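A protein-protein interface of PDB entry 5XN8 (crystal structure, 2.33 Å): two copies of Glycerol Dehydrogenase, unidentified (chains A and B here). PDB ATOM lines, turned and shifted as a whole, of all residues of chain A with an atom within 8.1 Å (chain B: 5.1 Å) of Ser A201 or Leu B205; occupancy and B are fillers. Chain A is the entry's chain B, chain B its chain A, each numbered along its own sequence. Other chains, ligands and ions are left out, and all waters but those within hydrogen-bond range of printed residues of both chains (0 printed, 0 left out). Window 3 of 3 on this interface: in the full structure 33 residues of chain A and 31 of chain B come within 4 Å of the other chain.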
ATOM      1  N   TRP A 176     -13.169 -10.364  -3.872  1.00  0.00           N
ATOM      2  CA  TRP A 176     -12.278 -10.012  -2.753  1.00  0.00           C
ATOM      3  C   TRP A 176     -10.870 -10.578  -2.906  1.00  0.00           C
ATOM      4  O   TRP A 176      -9.889  -9.892  -2.619  1.00  0.00           O
ATOM      5  CB  TRP A 176     -12.869 -10.481  -1.416  1.00  0.00           C
ATOM      6  CG  TRP A 176     -11.881 -10.468  -0.293  1.00  0.00           C
ATOM      7  CD1 TRP A 176     -11.473 -11.531   0.433  1.00  0.00           C
ATOM      8  CD2 TRP A 176     -11.157  -9.337   0.203  1.00  0.00           C
ATOM      9  NE1 TRP A 176     -10.540 -11.146   1.361  1.00  0.00           N
ATOM     10  CE2 TRP A 176     -10.329  -9.798   1.242  1.00  0.00           C
ATOM     11  CE3 TRP A 176     -11.126  -7.974  -0.133  1.00  0.00           C
ATOM     12  CZ2 TRP A 176      -9.485  -8.947   1.964  1.00  0.00           C
ATOM     13  CZ3 TRP A 176     -10.286  -7.132   0.577  1.00  0.00           C
ATOM     14  CH2 TRP A 176      -9.479  -7.619   1.618  1.00  0.00           C
ATOM     15  N   ALA A 179      -9.129  -8.925  -6.009  1.00  0.00           N
ATOM     16  CA  ALA A 179      -8.943  -7.507  -5.693  1.00  0.00           C
ATOM     17  C   ALA A 179      -7.787  -7.364  -4.722  1.00  0.00           C
ATOM     18  O   ALA A 179      -6.820  -6.657  -5.008  1.00  0.00           O
ATOM     19  CB  ALA A 179     -10.209  -6.920  -5.104  1.00  0.00           C
ATOM     20  N   TYR A 183      -4.214  -5.530  -4.996  1.00  0.00           N
ATOM     21  CA  TYR A 183      -3.859  -4.492  -4.022  1.00  0.00           C
ATOM     22  C   TYR A 183      -2.484  -4.765  -3.410  1.00  0.00           C
ATOM     23  O   TYR A 183      -1.629  -3.871  -3.379  1.00  0.00           O
ATOM     24  CB  TYR A 183      -4.930  -4.402  -2.934  1.00  0.00           C
ATOM     25  CG  TYR A 183      -4.730  -3.310  -1.908  1.00  0.00           C
ATOM     26  CD1 TYR A 183      -4.889  -1.963  -2.247  1.00  0.00           C
ATOM     27  CD2 TYR A 183      -4.401  -3.621  -0.587  1.00  0.00           C
ATOM     28  CE1 TYR A 183      -4.709  -0.957  -1.302  1.00  0.00           C
ATOM     29  CE2 TYR A 183      -4.221  -2.629   0.367  1.00  0.00           C
ATOM     30  CZ  TYR A 183      -4.381  -1.297   0.007  1.00  0.00           C
ATOM     31  OH  TYR A 183      -4.211  -0.322   0.957  1.00  0.00           O
ATOM     32  N   SER A 195      -5.632   0.634  -6.857  1.00  0.00           N
ATOM     33  CA  SER A 195      -6.951   0.580  -6.246  1.00  0.00           C
ATOM     34  C   SER A 195      -7.135   1.681  -5.216  1.00  0.00           C
ATOM     35  O   SER A 195      -6.237   1.972  -4.414  1.00  0.00           O
ATOM     36  CB  SER A 195      -7.213  -0.765  -5.575  1.00  0.00           C
ATOM     37  OG  SER A 195      -8.587  -0.870  -5.217  1.00  0.00           O
ATOM     38  N   THR A 196      -8.314   2.291  -5.250  1.00  0.00           N
ATOM     39  CA  THR A 196      -8.785   3.119  -4.162  1.00  0.00           C
ATOM     40  C   THR A 196      -9.160   2.191  -3.017  1.00  0.00           C
ATOM     41  O   THR A 196      -9.364   0.986  -3.232  1.00  0.00           O
ATOM     42  CB  THR A 196     -10.027   3.939  -4.578  1.00  0.00           C
ATOM     43  OG1 THR A 196     -11.059   3.054  -5.042  1.00  0.00           O
ATOM     44  CG2 THR A 196      -9.673   4.939  -5.675  1.00  0.00           C
ATOM     45  N   GLU A 197      -9.241   2.728  -1.801  1.00  0.00           N
ATOM     46  CA  GLU A 197      -9.751   1.956  -0.667  1.00  0.00           C
ATOM     47  C   GLU A 197     -11.234   1.652  -0.854  1.00  0.00           C
ATOM     48  O   GLU A 197     -11.694   0.580  -0.459  1.00  0.00           O
ATOM     49  CB  GLU A 197      -9.537   2.696   0.654  1.00  0.00           C
ATOM     50  CG  GLU A 197      -8.078   2.931   1.028  1.00  0.00           C
ATOM     51  CD  GLU A 197      -7.246   1.657   1.038  1.00  0.00           C
ATOM     52  OE1 GLU A 197      -7.716   0.646   1.569  1.00  0.00           O
ATOM     53  OE2 GLU A 197      -6.111   1.671   0.517  1.00  0.00           O
ATOM     54  N   ALA A 198     -11.961   2.596  -1.461  1.00  0.00           N
ATOM     55  CA  ALA A 198     -13.379   2.438  -1.803  1.00  0.00           C
ATOM     56  C   ALA A 198     -13.679   1.132  -2.537  1.00  0.00           C
ATOM     57  O   ALA A 198     -14.529   0.348  -2.109  1.00  0.00           O
ATOM     58  CB  ALA A 198     -13.838   3.613  -2.652  1.00  0.00           C
ATOM     59  N   ALA A 199     -12.970   0.920  -3.641  1.00  0.00           N
ATOM     60  CA  ALA A 199     -13.140  -0.258  -4.492  1.00  0.00           C
ATOM     61  C   ALA A 199     -12.786  -1.558  -3.776  1.00  0.00           C
ATOM     62  O   ALA A 199     -13.493  -2.560  -3.912  1.00  0.00           O
ATOM     63  CB  ALA A 199     -12.305  -0.101  -5.750  1.00  0.00           C
ATOM     64  N   LEU A 200     -11.687  -1.535  -3.024  1.00  0.00           N
ATOM     65  CA  LEU A 200     -11.257  -2.690  -2.222  1.00  0.00           C
ATOM     66  C   LEU A 200     -12.207  -2.990  -1.065  1.00  0.00           C
ATOM     67  O   LEU A 200     -12.442  -4.154  -0.742  1.00  0.00           O
ATOM     68  CB  LEU A 200      -9.846  -2.457  -1.673  1.00  0.00           C
ATOM     69  CG  LEU A 200      -9.218  -3.579  -0.838  1.00  0.00           C
ATOM     70  CD1 LEU A 200      -8.827  -4.737  -1.729  1.00  0.00           C
ATOM     71  CD2 LEU A 200      -8.016  -3.057  -0.067  1.00  0.00           C
ATOM     72  N   SER A 201     -12.722  -1.948  -0.421  1.00  0.00           N
ATOM     73  CA  SER A 201     -13.713  -2.105   0.651  1.00  0.00           C
ATOM     74  C   SER A 201     -14.987  -2.767   0.145  1.00  0.00           C
ATOM     75  O   SER A 201     -15.556  -3.616   0.831  1.00  0.00           O
ATOM     76  CB  SER A 201     -14.056  -0.745   1.266  1.00  0.00           C
ATOM     77  OG  SER A 201     -15.316  -0.719   1.914  1.00  0.00           O
ATOM     78  N   LEU A 202     -15.440  -2.361  -1.048  1.00  0.00           N
ATOM     79  CA  LEU A 202     -16.630  -2.944  -1.673  1.00  0.00           C
ATOM     80  C   LEU A 202     -16.383  -4.379  -2.139  1.00  0.00           C
ATOM     81  O   LEU A 202     -17.282  -5.221  -2.079  1.00  0.00           O
ATOM     82  CB  LEU A 202     -17.110  -2.084  -2.840  1.00  0.00           C
ATOM     83  CG  LEU A 202     -17.729  -0.727  -2.530  1.00  0.00           C
ATOM     84  CD1 LEU A 202     -17.914   0.061  -3.812  1.00  0.00           C
ATOM     85  CD2 LEU A 202     -19.074  -0.858  -1.799  1.00  0.00           C
ATOM     86  N   ALA A 203     -15.167  -4.647  -2.600  1.00  0.00           N
ATOM     87  CA  ALA A 203     -14.707  -6.019  -2.854  1.00  0.00           C
ATOM     88  C   ALA A 203     -14.845  -6.916  -1.626  1.00  0.00           C
ATOM     89  O   ALA A 203     -15.299  -8.044  -1.749  1.00  0.00           O
ATOM     90  CB  ALA A 203     -13.260  -6.019  -3.331  1.00  0.00           C
ATOM     91  N   ARG A 204     -14.460  -6.406  -0.458  1.00  0.00           N
ATOM     92  CA  ARG A 204     -14.542  -7.149   0.805  1.00  0.00           C
ATOM     93  C   ARG A 204     -15.976  -7.290   1.269  1.00  0.00           C
ATOM     94  O   ARG A 204     -16.370  -8.349   1.751  1.00  0.00           O
ATOM     95  CB  ARG A 204     -13.710  -6.461   1.906  1.00  0.00           C
ATOM     96  CG  ARG A 204     -13.704  -7.166   3.264  1.00  0.00           C
ATOM     97  CD  ARG A 204     -12.896  -8.465   3.271  1.00  0.00           C
ATOM     98  NE  ARG A 204     -13.412  -9.425   4.254  1.00  0.00           N
ATOM     99  CZ  ARG A 204     -12.720 -10.412   4.833  1.00  0.00           C
ATOM    100  NH1 ARG A 204     -11.436 -10.630   4.557  1.00  0.00           N
ATOM    101  NH2 ARG A 204     -13.340 -11.210   5.707  1.00  0.00           N
ATOM    102  N   LEU A 205     -16.751  -6.219   1.152  1.00  0.00           N
ATOM    103  CA  LEU A 205     -18.173  -6.263   1.483  1.00  0.00           C
ATOM    104  C   LEU A 205     -18.912  -7.307   0.635  1.00  0.00           C
ATOM    105  O   LEU A 205     -19.798  -7.998   1.129  1.00  0.00           O
ATOM    106  CB  LEU A 205     -18.813  -4.889   1.284  1.00  0.00           C
ATOM    107  CG  LEU A 205     -20.290  -4.784   1.691  1.00  0.00           C
ATOM    108  CD1 LEU A 205     -20.461  -4.966   3.198  1.00  0.00           C
ATOM    109  CD2 LEU A 205     -20.852  -3.446   1.224  1.00  0.00           C
ATOM    110  N   CYS A 206     -18.557  -7.400  -0.638  1.00  0.00           N
ATOM    111  CA  CYS A 206     -19.084  -8.454  -1.516  1.00  0.00           C
ATOM    112  C   CYS A 206     -18.953  -9.836  -0.863  1.00  0.00           C
ATOM    113  O   CYS A 206     -19.937 -10.570  -0.727  1.00  0.00           O
ATOM    114  CB  CYS A 206     -18.334  -8.437  -2.850  1.00  0.00           C
ATOM    115  SG  CYS A 206     -18.960  -9.591  -4.072  1.00  0.00           S
ATOM    116  N   TYR A 207     -17.732 -10.146  -0.425  1.00  0.00           N
ATOM    117  CA  TYR A 207     -17.390 -11.430   0.187  1.00  0.00           C
ATOM    118  C   TYR A 207     -18.127 -11.676   1.501  1.00  0.00           C
ATOM    119  O   TYR A 207     -18.680 -12.761   1.691  1.00  0.00           O
ATOM    120  CB  TYR A 207     -15.869 -11.516   0.393  1.00  0.00           C
ATOM    121  CG  TYR A 207     -15.371 -12.759   1.091  1.00  0.00           C
ATOM    122  CD1 TYR A 207     -15.526 -14.025   0.516  1.00  0.00           C
ATOM    123  CD2 TYR A 207     -14.724 -12.672   2.316  1.00  0.00           C
ATOM    124  CE1 TYR A 207     -15.063 -15.155   1.150  1.00  0.00           C
ATOM    125  CE2 TYR A 207     -14.254 -13.804   2.962  1.00  0.00           C
ATOM    126  CZ  TYR A 207     -14.422 -15.039   2.377  1.00  0.00           C
ATOM    127  OH  TYR A 207     -13.953 -16.158   3.029  1.00  0.00           O
ATOM    128  N   ASP A 208     -18.146 -10.682   2.397  1.00  0.00           N
ATOM    129  CA  ASP A 208     -18.845 -10.819   3.690  1.00  0.00           C
ATOM    130  C   ASP A 208     -20.359 -10.956   3.511  1.00  0.00           C
ATOM    131  O   ASP A 208     -21.020 -11.644   4.299  1.00  0.00           O
ATOM    132  CB  ASP A 208     -18.559  -9.642   4.629  1.00  0.00           C
ATOM    133  CG  ASP A 208     -17.091  -9.542   5.046  1.00  0.00           C
ATOM    134  OD1 ASP A 208     -16.401 -10.575   5.154  1.00  0.00           O
ATOM    135  OD2 ASP A 208     -16.623  -8.398   5.277  1.00  0.00           O
ATOM    136  N   LEU A 240     -21.389  -4.551  -6.118  1.00  0.00           N
ATOM    137  CA  LEU A 240     -20.202  -4.731  -5.282  1.00  0.00           C
ATOM    138  C   LEU A 240     -19.103  -5.513  -6.006  1.00  0.00           C
ATOM    139  O   LEU A 240     -17.906  -5.189  -5.882  1.00  0.00           O
ATOM    140  CB  LEU A 240     -20.536  -5.435  -3.966  1.00  0.00           C
ATOM    141  CG  LEU A 240     -21.631  -4.850  -3.056  1.00  0.00           C
ATOM    142  CD1 LEU A 240     -21.685  -5.588  -1.729  1.00  0.00           C
ATOM    143  CD2 LEU A 240     -21.446  -3.374  -2.830  1.00  0.00           C
ATOM    144  N   ILE A 243     -17.827  -3.172  -9.325  1.00  0.00           N
ATOM    145  CA  ILE A 243     -16.845  -2.143  -8.944  1.00  0.00           C
ATOM    146  C   ILE A 243     -15.562  -2.835  -8.487  1.00  0.00           C
ATOM    147  O   ILE A 243     -14.458  -2.395  -8.818  1.00  0.00           O
ATOM    148  CB  ILE A 243     -17.360  -1.203  -7.812  1.00  0.00           C
ATOM    149  CG1 ILE A 243     -18.613  -0.419  -8.240  1.00  0.00           C
ATOM    150  CG2 ILE A 243     -16.270  -0.227  -7.365  1.00  0.00           C
ATOM    151  CD1 ILE A 243     -18.430   0.525  -9.407  1.00  0.00           C
ATOM    152  N   GLY A 244     -15.723  -3.917  -7.726  1.00  0.00           N
ATOM    153  CA  GLY A 244     -14.610  -4.720  -7.251  1.00  0.00           C
ATOM    154  C   GLY A 244     -13.632  -5.216  -8.302  1.00  0.00           C
ATOM    155  O   GLY A 244     -12.435  -5.046  -8.141  1.00  0.00           O
ATOM    156  N   SER A 248     -10.651  -2.535  -8.734  1.00  0.00           N
ATOM    157  CA  SER A 248      -9.664  -3.093  -7.793  1.00  0.00           C
ATOM    158  C   SER A 248      -8.748  -4.097  -8.513  1.00  0.00           C
ATOM    159  O   SER A 248      -7.528  -4.001  -8.387  1.00  0.00           O
ATOM    160  CB  SER A 248     -10.353  -3.713  -6.578  1.00  0.00           C
ATOM    161  OG  SER A 248      -9.675  -3.394  -5.378  1.00  0.00           O
ATOM    162  N   SER B 201     -21.884   1.447   3.546  1.00  0.00           N
ATOM    163  CA  SER B 201     -20.566   0.889   3.875  1.00  0.00           C
ATOM    164  C   SER B 201     -19.455   1.920   3.672  1.00  0.00           C
ATOM    165  O   SER B 201     -18.534   1.997   4.476  1.00  0.00           O
ATOM    166  CB  SER B 201     -20.276  -0.341   3.023  1.00  0.00           C
ATOM    167  OG  SER B 201     -19.914   0.060   1.720  1.00  0.00           O
ATOM    168  N   LEU B 202     -19.541   2.690   2.588  1.00  0.00           N
ATOM    169  CA  LEU B 202     -18.564   3.755   2.296  1.00  0.00           C
ATOM    170  C   LEU B 202     -18.697   4.928   3.261  1.00  0.00           C
ATOM    171  O   LEU B 202     -17.698   5.549   3.630  1.00  0.00           O
ATOM    172  CB  LEU B 202     -18.700   4.247   0.852  1.00  0.00           C
ATOM    173  CG  LEU B 202     -18.270   3.301  -0.267  1.00  0.00           C
ATOM    174  CD1 LEU B 202     -18.703   3.886  -1.603  1.00  0.00           C
ATOM    175  CD2 LEU B 202     -16.780   3.011  -0.284  1.00  0.00           C
ATOM    176  N   ALA B 203     -19.927   5.218   3.673  1.00  0.00           N
ATOM    177  CA  ALA B 203     -20.188   6.146   4.779  1.00  0.00           C
ATOM    178  C   ALA B 203     -19.456   5.744   6.057  1.00  0.00           C
ATOM    179  O   ALA B 203     -18.871   6.597   6.720  1.00  0.00           O
ATOM    180  CB  ALA B 203     -21.679   6.247   5.050  1.00  0.00           C
ATOM    181  N   ARG B 204     -19.487   4.455   6.392  1.00  0.00           N
ATOM    182  CA  ARG B 204     -18.825   3.922   7.584  1.00  0.00           C
ATOM    183  C   ARG B 204     -17.317   3.912   7.425  1.00  0.00           C
ATOM    184  O   ARG B 204     -16.592   4.242   8.360  1.00  0.00           O
ATOM    185  CB  ARG B 204     -19.319   2.492   7.901  1.00  0.00           C
ATOM    186  CG  ARG B 204     -18.707   1.843   9.145  1.00  0.00           C
ATOM    187  CD  ARG B 204     -19.214   2.459  10.453  1.00  0.00           C
ATOM    188  NE  ARG B 204     -18.212   2.380  11.526  1.00  0.00           N
ATOM    189  CZ  ARG B 204     -18.455   2.380  12.835  1.00  0.00           C
ATOM    190  NH1 ARG B 204     -19.694   2.457  13.324  1.00  0.00           N
ATOM    191  NH2 ARG B 204     -17.438   2.292  13.685  1.00  0.00           N
ATOM    192  N   LEU B 205     -16.848   3.516   6.247  1.00  0.00           N
ATOM    193  CA  LEU B 205     -15.421   3.552   5.944  1.00  0.00           C
ATOM    194  C   LEU B 205     -14.855   4.963   6.067  1.00  0.00           C
ATOM    195  O   LEU B 205     -13.737   5.150   6.541  1.00  0.00           O
ATOM    196  CB  LEU B 205     -15.154   3.004   4.540  1.00  0.00           C
ATOM    197  CG  LEU B 205     -13.680   2.890   4.143  1.00  0.00           C
ATOM    198  CD1 LEU B 205     -12.963   1.853   4.994  1.00  0.00           C
ATOM    199  CD2 LEU B 205     -13.567   2.568   2.667  1.00  0.00           C
ATOM    200  N   CYS B 206     -15.612   5.951   5.615  1.00  0.00           N
ATOM    201  CA  CYS B 206     -15.247   7.362   5.806  1.00  0.00           C
ATOM    202  C   CYS B 206     -14.878   7.646   7.264  1.00  0.00           C
ATOM    203  O   CYS B 206     -13.786   8.159   7.555  1.00  0.00           O
ATOM    204  CB  CYS B 206     -16.411   8.253   5.380  1.00  0.00           C
ATOM    205  SG  CYS B 206     -16.073  10.003   5.428  1.00  0.00           S
ATOM    206  N   TYR B 207     -15.780   7.262   8.168  1.00  0.00           N
ATOM    207  CA  TYR B 207     -15.634   7.486   9.603  1.00  0.00           C
ATOM    208  C   TYR B 207     -14.449   6.735  10.204  1.00  0.00           C
ATOM    209  O   TYR B 207     -13.672   7.330  10.954  1.00  0.00           O
ATOM    210  CB  TYR B 207     -16.945   7.104  10.321  1.00  0.00           C
ATOM    211  CG  TYR B 207     -16.918   7.203  11.832  1.00  0.00           C
ATOM    212  CD1 TYR B 207     -16.727   8.429  12.471  1.00  0.00           C
ATOM    213  CD2 TYR B 207     -17.093   6.074  12.619  1.00  0.00           C
ATOM    214  CE1 TYR B 207     -16.709   8.522  13.851  1.00  0.00           C
ATOM    215  CE2 TYR B 207     -17.078   6.149  14.000  1.00  0.00           C
ATOM    216  CZ  TYR B 207     -16.874   7.379  14.614  1.00  0.00           C
ATOM    217  OH  TYR B 207     -16.838   7.472  15.991  1.00  0.00           O
ATOM    218  N   ASP B 208     -14.299   5.448   9.879  1.00  0.00           N
ATOM    219  CA  ASP B 208     -13.172   4.644  10.394  1.00  0.00           C
ATOM    220  C   ASP B 208     -11.829   5.137   9.867  1.00  0.00           C
ATOM    221  O   ASP B 208     -10.814   5.035  10.554  1.00  0.00           O
ATOM    222  CB  ASP B 208     -13.323   3.150  10.046  1.00  0.00           C
ATOM    223  CG  ASP B 208     -14.538   2.499  10.712  1.00  0.00           C
ATOM    224  OD1 ASP B 208     -14.943   2.910  11.829  1.00  0.00           O
ATOM    225  OD2 ASP B 208     -15.092   1.555  10.106  1.00  0.00           O
ATOM    226  N   THR B 209     -11.826   5.633   8.635  1.00  0.00           N
ATOM    227  CA  THR B 209     -10.628   6.207   8.018  1.00  0.00           C
ATOM    228  C   THR B 209     -10.202   7.502   8.720  1.00  0.00           C
ATOM    229  O   THR B 209      -9.020   7.700   8.962  1.00  0.00           O
ATOM    230  CB  THR B 209     -10.832   6.455   6.508  1.00  0.00           C
ATOM    231  OG1 THR B 209     -11.181   5.227   5.872  1.00  0.00           O
ATOM    232  CG2 THR B 209      -9.575   7.000   5.856  1.00  0.00           C
ATOM    233  N   LEU B 210     -11.152   8.364   9.063  1.00  0.00           N
ATOM    234  CA  LEU B 210     -10.827   9.580   9.839  1.00  0.00           C
ATOM    235  C   LEU B 210     -10.141   9.238  11.160  1.00  0.00           C
ATOM    236  O   LEU B 210      -9.112   9.826  11.483  1.00  0.00           O
ATOM    237  CB  LEU B 210     -12.060  10.421  10.130  1.00  0.00           C
ATOM    238  CG  LEU B 210     -12.726  11.145   8.976  1.00  0.00           C
ATOM    239  CD1 LEU B 210     -14.016  11.803   9.435  1.00  0.00           C
ATOM    240  CD2 LEU B 210     -11.800  12.173   8.371  1.00  0.00           C
ATOM    241  N   LEU B 240     -15.493   9.081  -0.429  1.00  0.00           N
ATOM    242  CA  LEU B 240     -16.255   8.314   0.565  1.00  0.00           C
ATOM    243  C   LEU B 240     -17.369   9.144   1.201  1.00  0.00           C
ATOM    244  O   LEU B 240     -18.475   8.632   1.439  1.00  0.00           O
ATOM    245  CB  LEU B 240     -15.345   7.760   1.672  1.00  0.00           C
ATOM    246  CG  LEU B 240     -14.136   6.904   1.284  1.00  0.00           C
ATOM    247  CD1 LEU B 240     -13.486   6.305   2.521  1.00  0.00           C
ATOM    248  CD2 LEU B 240     -14.556   5.788   0.325  1.00  0.00           C
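Ser A201 touches Leu B205, and with the chains exchanged Leu A205 touches Ser B201.
Leu A202 touches Ser B201, but with the chains exchanged Ser A201 does not touch Leu B202 (4.6 Å).
9 positions are printed for both chains.
Hydrophobic or aromatic side chains of chain B within 4 Å of the printed part of chain A: Leu B202, Leu B205 and Leu B240.
Hydrophobic or aromatic side chains of chain A that line the printed part of chain B: Ala A198, Leu A202 and Leu A205.
Among the printed residues, 5 pairs touch across the chains.
Among the printed residues, no Asp or Glu carboxylate lies within 4 Å of a Lys or Arg side-chain nitrogen of the other chain.
Among the printed residues, pairs that only touch across the chains: Ser A201 with Leu B205 (3.6 Å), Leu A205 with Ser B201 (3.6 Å), Leu A202 with Ser B201 (3.7 Å), Ala A198 with Leu B240 (3.8 Å) and Ala A198 with Leu B202 (3.8 Å).
O of Leu B205 sits at hydrogen-bond distance from OG1 of Thr B209 (2.6 Å).
Of chain B, only Leu B205 (3.6 Å) comes within 4 Å of Ser A201.
Of the printed residues of chain A, Leu B205 touches Ser A201 (3.6 Å).
Of the printed residues of chain A, Leu B202 touches Ala A198 (3.8 Å).
Of the printed residues of chain B, Leu A205 touches Ser B201.
Of the printed residues of chain A, Ser B201 touches Leu A202 and Leu A205.
Printed residues of chain B within 4 Å of Leu A202: Ser B201.
The nearest residue of chain A that does not touch Leu B205 is Glu A197 (4.2 Å).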
